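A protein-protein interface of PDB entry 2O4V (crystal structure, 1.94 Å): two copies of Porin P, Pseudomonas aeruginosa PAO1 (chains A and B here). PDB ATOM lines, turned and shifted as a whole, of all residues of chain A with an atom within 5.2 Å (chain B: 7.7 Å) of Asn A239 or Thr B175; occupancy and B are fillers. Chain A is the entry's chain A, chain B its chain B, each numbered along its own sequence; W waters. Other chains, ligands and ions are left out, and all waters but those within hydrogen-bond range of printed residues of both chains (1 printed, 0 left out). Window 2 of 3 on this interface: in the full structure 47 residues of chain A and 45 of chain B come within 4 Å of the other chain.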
ATOM      1  N   TYR A  46      15.428 -13.075  -3.601  1.00  0.00           N
ATOM      2  CA  TYR A  46      16.144 -12.297  -4.613  1.00  0.00           C
ATOM      3  C   TYR A  46      15.866 -12.690  -6.065  1.00  0.00           C
ATOM      4  O   TYR A  46      16.041 -11.872  -6.976  1.00  0.00           O
ATOM      5  CB  TYR A  46      17.647 -12.369  -4.357  1.00  0.00           C
ATOM      6  CG  TYR A  46      18.115 -11.596  -3.152  1.00  0.00           C
ATOM      7  CD1 TYR A  46      17.891 -10.222  -3.052  1.00  0.00           C
ATOM      8  CD2 TYR A  46      18.812 -12.231  -2.123  1.00  0.00           C
ATOM      9  CE1 TYR A  46      18.327  -9.505  -1.955  1.00  0.00           C
ATOM     10  CE2 TYR A  46      19.264 -11.519  -1.021  1.00  0.00           C
ATOM     11  CZ  TYR A  46      19.023 -10.153  -0.949  1.00  0.00           C
ATOM     12  OH  TYR A  46      19.472  -9.430   0.131  1.00  0.00           O
ATOM     13  N   THR A  47      15.462 -13.938  -6.283  1.00  0.00           N
ATOM     14  CA  THR A  47      15.148 -14.431  -7.624  1.00  0.00           C
ATOM     15  C   THR A  47      13.665 -14.813  -7.726  1.00  0.00           C
ATOM     16  O   THR A  47      13.005 -15.016  -6.709  1.00  0.00           O
ATOM     17  CB  THR A  47      16.047 -15.627  -8.036  1.00  0.00           C
ATOM     18  OG1 THR A  47      15.746 -16.762  -7.214  1.00  0.00           O
ATOM     19  CG2 THR A  47      17.540 -15.274  -7.887  1.00  0.00           C
ATOM     20  N   ASN A  48      13.147 -14.893  -8.951  1.00  0.00           N
ATOM     21  CA  ASN A  48      11.720 -15.175  -9.163  1.00  0.00           C
ATOM     22  C   ASN A  48      11.307 -16.597  -8.787  1.00  0.00           C
ATOM     23  O   ASN A  48      10.231 -16.800  -8.206  1.00  0.00           O
ATOM     24  CB  ASN A  48      11.301 -14.855 -10.603  1.00  0.00           C
ATOM     25  CG  ASN A  48      11.352 -13.369 -10.912  1.00  0.00           C
ATOM     26  OD1 ASN A  48      11.125 -12.531 -10.042  1.00  0.00           O
ATOM     27  ND2 ASN A  48      11.641 -13.037 -12.168  1.00  0.00           N
ATOM     28  N   ASN A  49      12.155 -17.575  -9.102  1.00  0.00           N
ATOM     29  CA  ASN A  49      11.867 -18.973  -8.763  1.00  0.00           C
ATOM     30  C   ASN A  49      12.563 -19.462  -7.489  1.00  0.00           C
ATOM     31  O   ASN A  49      12.367 -20.600  -7.071  1.00  0.00           O
ATOM     32  CB  ASN A  49      12.151 -19.908  -9.952  1.00  0.00           C
ATOM     33  CG  ASN A  49      13.619 -19.910 -10.375  1.00  0.00           C
ATOM     34  OD1 ASN A  49      14.512 -19.574  -9.594  1.00  0.00           O
ATOM     35  ND2 ASN A  49      13.870 -20.306 -11.616  1.00  0.00           N
ATOM     36  N   GLY A  50      13.374 -18.601  -6.878  1.00  0.00           N
ATOM     37  CA  GLY A  50      14.073 -18.943  -5.641  1.00  0.00           C
ATOM     38  C   GLY A  50      15.399 -19.664  -5.824  1.00  0.00           C
ATOM     39  O   GLY A  50      16.128 -19.867  -4.861  1.00  0.00           O
ATOM     40  N   ASN A  51      15.711 -20.056  -7.057  1.00  0.00           N
ATOM     41  CA  ASN A  51      16.996 -20.683  -7.368  1.00  0.00           C
ATOM     42  C   ASN A  51      18.125 -19.645  -7.441  1.00  0.00           C
ATOM     43  O   ASN A  51      17.871 -18.437  -7.431  1.00  0.00           O
ATOM     44  CB  ASN A  51      16.897 -21.486  -8.674  1.00  0.00           C
ATOM     45  CG  ASN A  51      15.970 -22.702  -8.555  1.00  0.00           C
ATOM     46  OD1 ASN A  51      15.745 -23.224  -7.465  1.00  0.00           O
ATOM     47  ND2 ASN A  51      15.424 -23.145  -9.687  1.00  0.00           N
ATOM     48  N   ALA A  53      20.867 -17.276  -8.849  1.00  0.00           N
ATOM     49  CA  ALA A  53      21.284 -16.508 -10.015  1.00  0.00           C
ATOM     50  C   ALA A  53      22.641 -15.889  -9.702  1.00  0.00           C
ATOM     51  O   ALA A  53      23.123 -15.971  -8.570  1.00  0.00           O
ATOM     52  CB  ALA A  53      20.264 -15.421 -10.321  1.00  0.00           C
ATOM     53  N   ALA A 236      20.655 -11.072 -13.034  1.00  0.00           N
ATOM     54  CA  ALA A 236      19.743 -12.225 -12.938  1.00  0.00           C
ATOM     55  C   ALA A 236      18.720 -12.286 -14.074  1.00  0.00           C
ATOM     56  O   ALA A 236      18.006 -13.283 -14.216  1.00  0.00           O
ATOM     57  CB  ALA A 236      19.035 -12.232 -11.581  1.00  0.00           C
ATOM     58  N   GLY A 237      18.653 -11.221 -14.873  1.00  0.00           N
ATOM     59  CA  GLY A 237      17.770 -11.142 -16.044  1.00  0.00           C
ATOM     60  C   GLY A 237      16.319 -11.466 -15.712  1.00  0.00           C
ATOM     61  O   GLY A 237      15.743 -10.891 -14.777  1.00  0.00           O
ATOM     62  N   SER A 238      15.745 -12.403 -16.467  1.00  0.00           N
ATOM     63  CA  SER A 238      14.360 -12.859 -16.275  1.00  0.00           C
ATOM     64  C   SER A 238      14.077 -13.541 -14.937  1.00  0.00           C
ATOM     65  O   SER A 238      12.914 -13.781 -14.599  1.00  0.00           O
ATOM     66  CB  SER A 238      13.962 -13.811 -17.404  1.00  0.00           C
ATOM     67  OG  SER A 238      13.907 -13.110 -18.628  1.00  0.00           O
ATOM     68  N   ASN A 239      15.125 -13.887 -14.194  1.00  0.00           N
ATOM     69  CA  ASN A 239      14.933 -14.516 -12.897  1.00  0.00           C
ATOM     70  C   ASN A 239      15.260 -13.583 -11.738  1.00  0.00           C
ATOM     71  O   ASN A 239      15.345 -14.019 -10.604  1.00  0.00           O
ATOM     72  CB  ASN A 239      15.724 -15.824 -12.795  1.00  0.00           C
ATOM     73  CG  ASN A 239      15.164 -16.767 -11.742  1.00  0.00           C
ATOM     74  OD1 ASN A 239      13.948 -16.870 -11.569  1.00  0.00           O
ATOM     75  ND2 ASN A 239      16.048 -17.462 -11.037  1.00  0.00           N
ATOM     76  N   GLY A 240      15.438 -12.296 -12.025  1.00  0.00           N
ATOM     77  CA  GLY A 240      15.717 -11.316 -10.978  1.00  0.00           C
ATOM     78  C   GLY A 240      14.438 -10.743 -10.398  1.00  0.00           C
ATOM     79  O   GLY A 240      13.595 -10.226 -11.138  1.00  0.00           O
ATOM     80  N   ASN A 241      14.293 -10.839  -9.078  1.00  0.00           N
ATOM     81  CA  ASN A 241      13.121 -10.310  -8.389  1.00  0.00           C
ATOM     82  C   ASN A 241      13.403  -8.937  -7.805  1.00  0.00           C
ATOM     83  O   ASN A 241      14.085  -8.806  -6.792  1.00  0.00           O
ATOM     84  CB  ASN A 241      12.632 -11.270  -7.292  1.00  0.00           C
ATOM     85  CG  ASN A 241      11.397 -10.743  -6.550  1.00  0.00           C
ATOM     86  OD1 ASN A 241      10.531 -10.091  -7.134  1.00  0.00           O
ATOM     87  ND2 ASN A 241      11.322 -11.026  -5.259  1.00  0.00           N
ATOM     88  N   ASN B 173      22.515 -16.130 -19.935  1.00  0.00           N
ATOM     89  CA  ASN B 173      21.948 -16.700 -18.712  1.00  0.00           C
ATOM     90  C   ASN B 173      21.310 -18.059 -18.938  1.00  0.00           C
ATOM     91  O   ASN B 173      20.770 -18.317 -20.019  1.00  0.00           O
ATOM     92  CB  ASN B 173      20.846 -15.785 -18.173  1.00  0.00           C
ATOM     93  CG  ASN B 173      21.357 -14.720 -17.220  1.00  0.00           C
ATOM     94  OD1 ASN B 173      20.619 -13.790 -16.893  1.00  0.00           O
ATOM     95  ND2 ASN B 173      22.590 -14.856 -16.749  1.00  0.00           N
ATOM     96  N   ASP B 174      21.341 -18.918 -17.915  1.00  0.00           N
ATOM     97  CA  ASP B 174      20.438 -20.074 -17.910  1.00  0.00           C
ATOM     98  C   ASP B 174      19.074 -19.636 -17.365  1.00  0.00           C
ATOM     99  O   ASP B 174      18.875 -18.449 -17.069  1.00  0.00           O
ATOM    100  CB  ASP B 174      21.030 -21.312 -17.193  1.00  0.00           C
ATOM    101  CG  ASP B 174      21.183 -21.139 -15.678  1.00  0.00           C
ATOM    102  OD1 ASP B 174      20.599 -20.212 -15.082  1.00  0.00           O
ATOM    103  OD2 ASP B 174      21.897 -21.972 -15.072  1.00  0.00           O
ATOM    104  N   THR B 175      18.147 -20.581 -17.234  1.00  0.00           N
ATOM    105  CA  THR B 175      16.778 -20.275 -16.790  1.00  0.00           C
ATOM    106  C   THR B 175      16.720 -19.723 -15.358  1.00  0.00           C
ATOM    107  O   THR B 175      15.764 -19.038 -14.991  1.00  0.00           O
ATOM    108  CB  THR B 175      15.848 -21.505 -16.916  1.00  0.00           C
ATOM    109  OG1 THR B 175      16.384 -22.589 -16.151  1.00  0.00           O
ATOM    110  CG2 THR B 175      15.731 -21.942 -18.367  1.00  0.00           C
ATOM    111  N   ASP B 176      17.742 -20.017 -14.556  1.00  0.00           N
ATOM    112  CA  ASP B 176      17.835 -19.476 -13.203  1.00  0.00           C
ATOM    113  C   ASP B 176      18.531 -18.105 -13.135  1.00  0.00           C
ATOM    114  O   ASP B 176      18.676 -17.535 -12.053  1.00  0.00           O
ATOM    115  CB  ASP B 176      18.519 -20.483 -12.271  1.00  0.00           C
ATOM    116  CG  ASP B 176      17.696 -21.750 -12.071  1.00  0.00           C
ATOM    117  OD1 ASP B 176      16.442 -21.695 -12.168  1.00  0.00           O
ATOM    118  OD2 ASP B 176      18.305 -22.810 -11.802  1.00  0.00           O
ATOM    119  N   GLY B 177      18.941 -17.575 -14.290  1.00  0.00           N
ATOM    120  CA  GLY B 177      19.677 -16.309 -14.340  1.00  0.00           C
ATOM    121  C   GLY B 177      21.118 -16.460 -13.883  1.00  0.00           C
ATOM    122  O   GLY B 177      21.757 -15.494 -13.466  1.00  0.00           O
ATOM    123  N   ASP B 178      21.619 -17.692 -13.935  1.00  0.00           N
ATOM    124  CA  ASP B 178      23.019 -17.975 -13.651  1.00  0.00           C
ATOM    125  C   ASP B 178      23.769 -17.894 -14.986  1.00  0.00           C
ATOM    126  O   ASP B 178      23.335 -18.478 -15.980  1.00  0.00           O
ATOM    127  CB  ASP B 178      23.155 -19.366 -13.015  1.00  0.00           C
ATOM    128  CG  ASP B 178      24.510 -19.592 -12.344  1.00  0.00           C
ATOM    129  OD1 ASP B 178      25.299 -18.636 -12.184  1.00  0.00           O
ATOM    130  OD2 ASP B 178      24.785 -20.748 -11.961  1.00  0.00           O
ATOM    131  N   GLU B 211      23.687 -25.910 -21.030  1.00  0.00           N
ATOM    132  CA  GLU B 211      22.474 -26.538 -20.510  1.00  0.00           C
ATOM    133  C   GLU B 211      21.488 -25.500 -19.983  1.00  0.00           C
ATOM    134  O   GLU B 211      21.825 -24.712 -19.099  1.00  0.00           O
ATOM    135  CB  GLU B 211      22.812 -27.561 -19.419  1.00  0.00           C
ATOM    136  CG  GLU B 211      23.449 -28.862 -19.940  1.00  0.00           C
ATOM    137  CD  GLU B 211      22.437 -29.958 -20.234  1.00  0.00           C
ATOM    138  OE1 GLU B 211      21.246 -29.639 -20.434  1.00  0.00           O
ATOM    139  OE2 GLU B 211      22.833 -31.149 -20.246  1.00  0.00           O
ATOM    140  N   ASP B 212      20.280 -25.515 -20.552  1.00  0.00           N
ATOM    141  CA  ASP B 212      19.174 -24.625 -20.171  1.00  0.00           C
ATOM    142  C   ASP B 212      19.507 -23.139 -20.308  1.00  0.00           C
ATOM    143  O   ASP B 212      19.004 -22.315 -19.545  1.00  0.00           O
ATOM    144  CB  ASP B 212      18.684 -24.929 -18.747  1.00  0.00           C
ATOM    145  CG  ASP B 212      18.182 -26.356 -18.586  1.00  0.00           C
ATOM    146  OD1 ASP B 212      17.424 -26.840 -19.460  1.00  0.00           O
ATOM    147  OD2 ASP B 212      18.539 -26.991 -17.568  1.00  0.00           O
ATOM    148  N   SER B 213      20.345 -22.804 -21.287  1.00  0.00           N
ATOM    149  CA  SER B 213      20.833 -21.438 -21.473  1.00  0.00           C
ATOM    150  C   SER B 213      20.406 -20.867 -22.812  1.00  0.00           C
ATOM    151  O   SER B 213      20.348 -21.587 -23.805  1.00  0.00           O
ATOM    152  CB  SER B 213      22.355 -21.407 -21.383  1.00  0.00           C
ATOM    153  OG  SER B 213      22.781 -21.686 -20.065  1.00  0.00           O
ATOM    154  N   ALA B 214      20.120 -19.567 -22.827  1.00  0.00           N
ATOM    155  CA  ALA B 214      19.731 -18.858 -24.044  1.00  0.00           C
ATOM    156  C   ALA B 214      20.953 -18.170 -24.636  1.00  0.00           C
ATOM    157  O   ALA B 214      21.468 -17.188 -24.069  1.00  0.00           O
ATOM    158  CB  ALA B 214      18.644 -17.846 -23.741  1.00  0.00           C
ATOM    159  N   GLU B 252      16.417 -20.806 -24.787  1.00  0.00           N
ATOM    160  CA  GLU B 252      16.830 -21.704 -23.705  1.00  0.00           C
ATOM    161  C   GLU B 252      16.548 -23.178 -24.024  1.00  0.00           C
ATOM    162  O   GLU B 252      15.448 -23.529 -24.449  1.00  0.00           O
ATOM    163  CB  GLU B 252      16.202 -21.269 -22.362  1.00  0.00           C
ATOM    164  CG  GLU B 252      17.173 -20.433 -21.498  1.00  0.00           C
ATOM    165  CD  GLU B 252      16.561 -19.212 -20.794  1.00  0.00           C
ATOM    166  OE1 GLU B 252      15.353 -19.231 -20.465  1.00  0.00           O
ATOM    167  OE2 GLU B 252      17.321 -18.229 -20.551  1.00  0.00           O
ATOM    168  N   GLY B 253      17.569 -24.018 -23.864  1.00  0.00           N
ATOM    169  CA  GLY B 253      17.420 -25.463 -23.984  1.00  0.00           C
ATOM    170  C   GLY B 253      17.669 -26.118 -25.334  1.00  0.00           C
ATOM    171  O   GLY B 253      17.404 -27.308 -25.493  1.00  0.00           O
HETATM  172  O   HOH W   1      17.772 -14.025 -18.007  1.00  0.00           O
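The side-chain carboxylate of Asp B176 sits at hydrogen-bond distance from the side-chain amide nitrogen of Asn A49 (3.0 Å). ND2 of Asn A51 lies within hydrogen-bond range of OD1 of Asp B176, 3.0 Å away. The side-chain amide nitrogen (ND2) of Asn A239 lies within hydrogen-bond range of the backbone carbonyl oxygen (O) of Asp B176, at 2.8 Å.
The backbone carbonyl oxygen (O) of Asn A51 lies within hydrogen-bond range of the side-chain hydroxyl (OG1) of Thr A47 (2.7 Å). The backbone NH (N) of Asn A48 is in hydrogen-bond range of the backbone carbonyl oxygen (O) of Asn A239. OD1 of Asn A49 lies within hydrogen-bond range of ND2 of Asn A239 (3.0 Å). The backbone NH (N) of Ala B214 sits at hydrogen-bond distance from the backbone carbonyl oxygen (O) of Asn B173. OD1 of Asp B174 is in hydrogen-bond range of N of Gly B177 (3.2 Å). The backbone NH (N) of Thr B175 sits at hydrogen-bond distance from the backbone carbonyl oxygen (O) of Asp B212 (3.0 Å).
Among the printed residues, merely in contact across the chains: Ala A53 with Asp B176, Ala A53 with Gly B177, Ala A236 with Asn B173, Ala A236 with Gly B177, Gly A237 with Asn B173, Asn A239 with Thr B175 and Asn A239 with Gly B177.
Printed residues of chain B within 4 Å of Asn A49: Asp B176. Printed residues of chain B within 4 Å of Asn A51: Asp B176 (3.0 Å). Gly B253 touches none of the printed residues of chain A. The nearest residue of chain A that does not touch Thr B175 is Asn A49 (4.1 Å). The nearest printed residue of chain B that does not touch Ala A236 is Asp B176 (4.8 Å).
Of the 12 printed residues of chain B, 4 touch a printed residue of chain A. Printed residues of chain A that touch a printed residue of chain B: Asn A49, Asn A51, Ala A53, Ala A236, Gly A237 and Asn A239. Hydrophobic or aromatic side chains of chain A within 4 Å of the printed part of chain B: Ala A53. Among the printed residues, no Asp or Glu carboxylate lies within 4 Å of a Lys or Arg side-chain nitrogen of the other chain.
No position is printed for both chains.
Water W1 bridges the backbone NH (N) of Ser A238 (3.0 Å) and the side-chain amide oxygen (OD1) of Asn B173 (3.1 Å).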
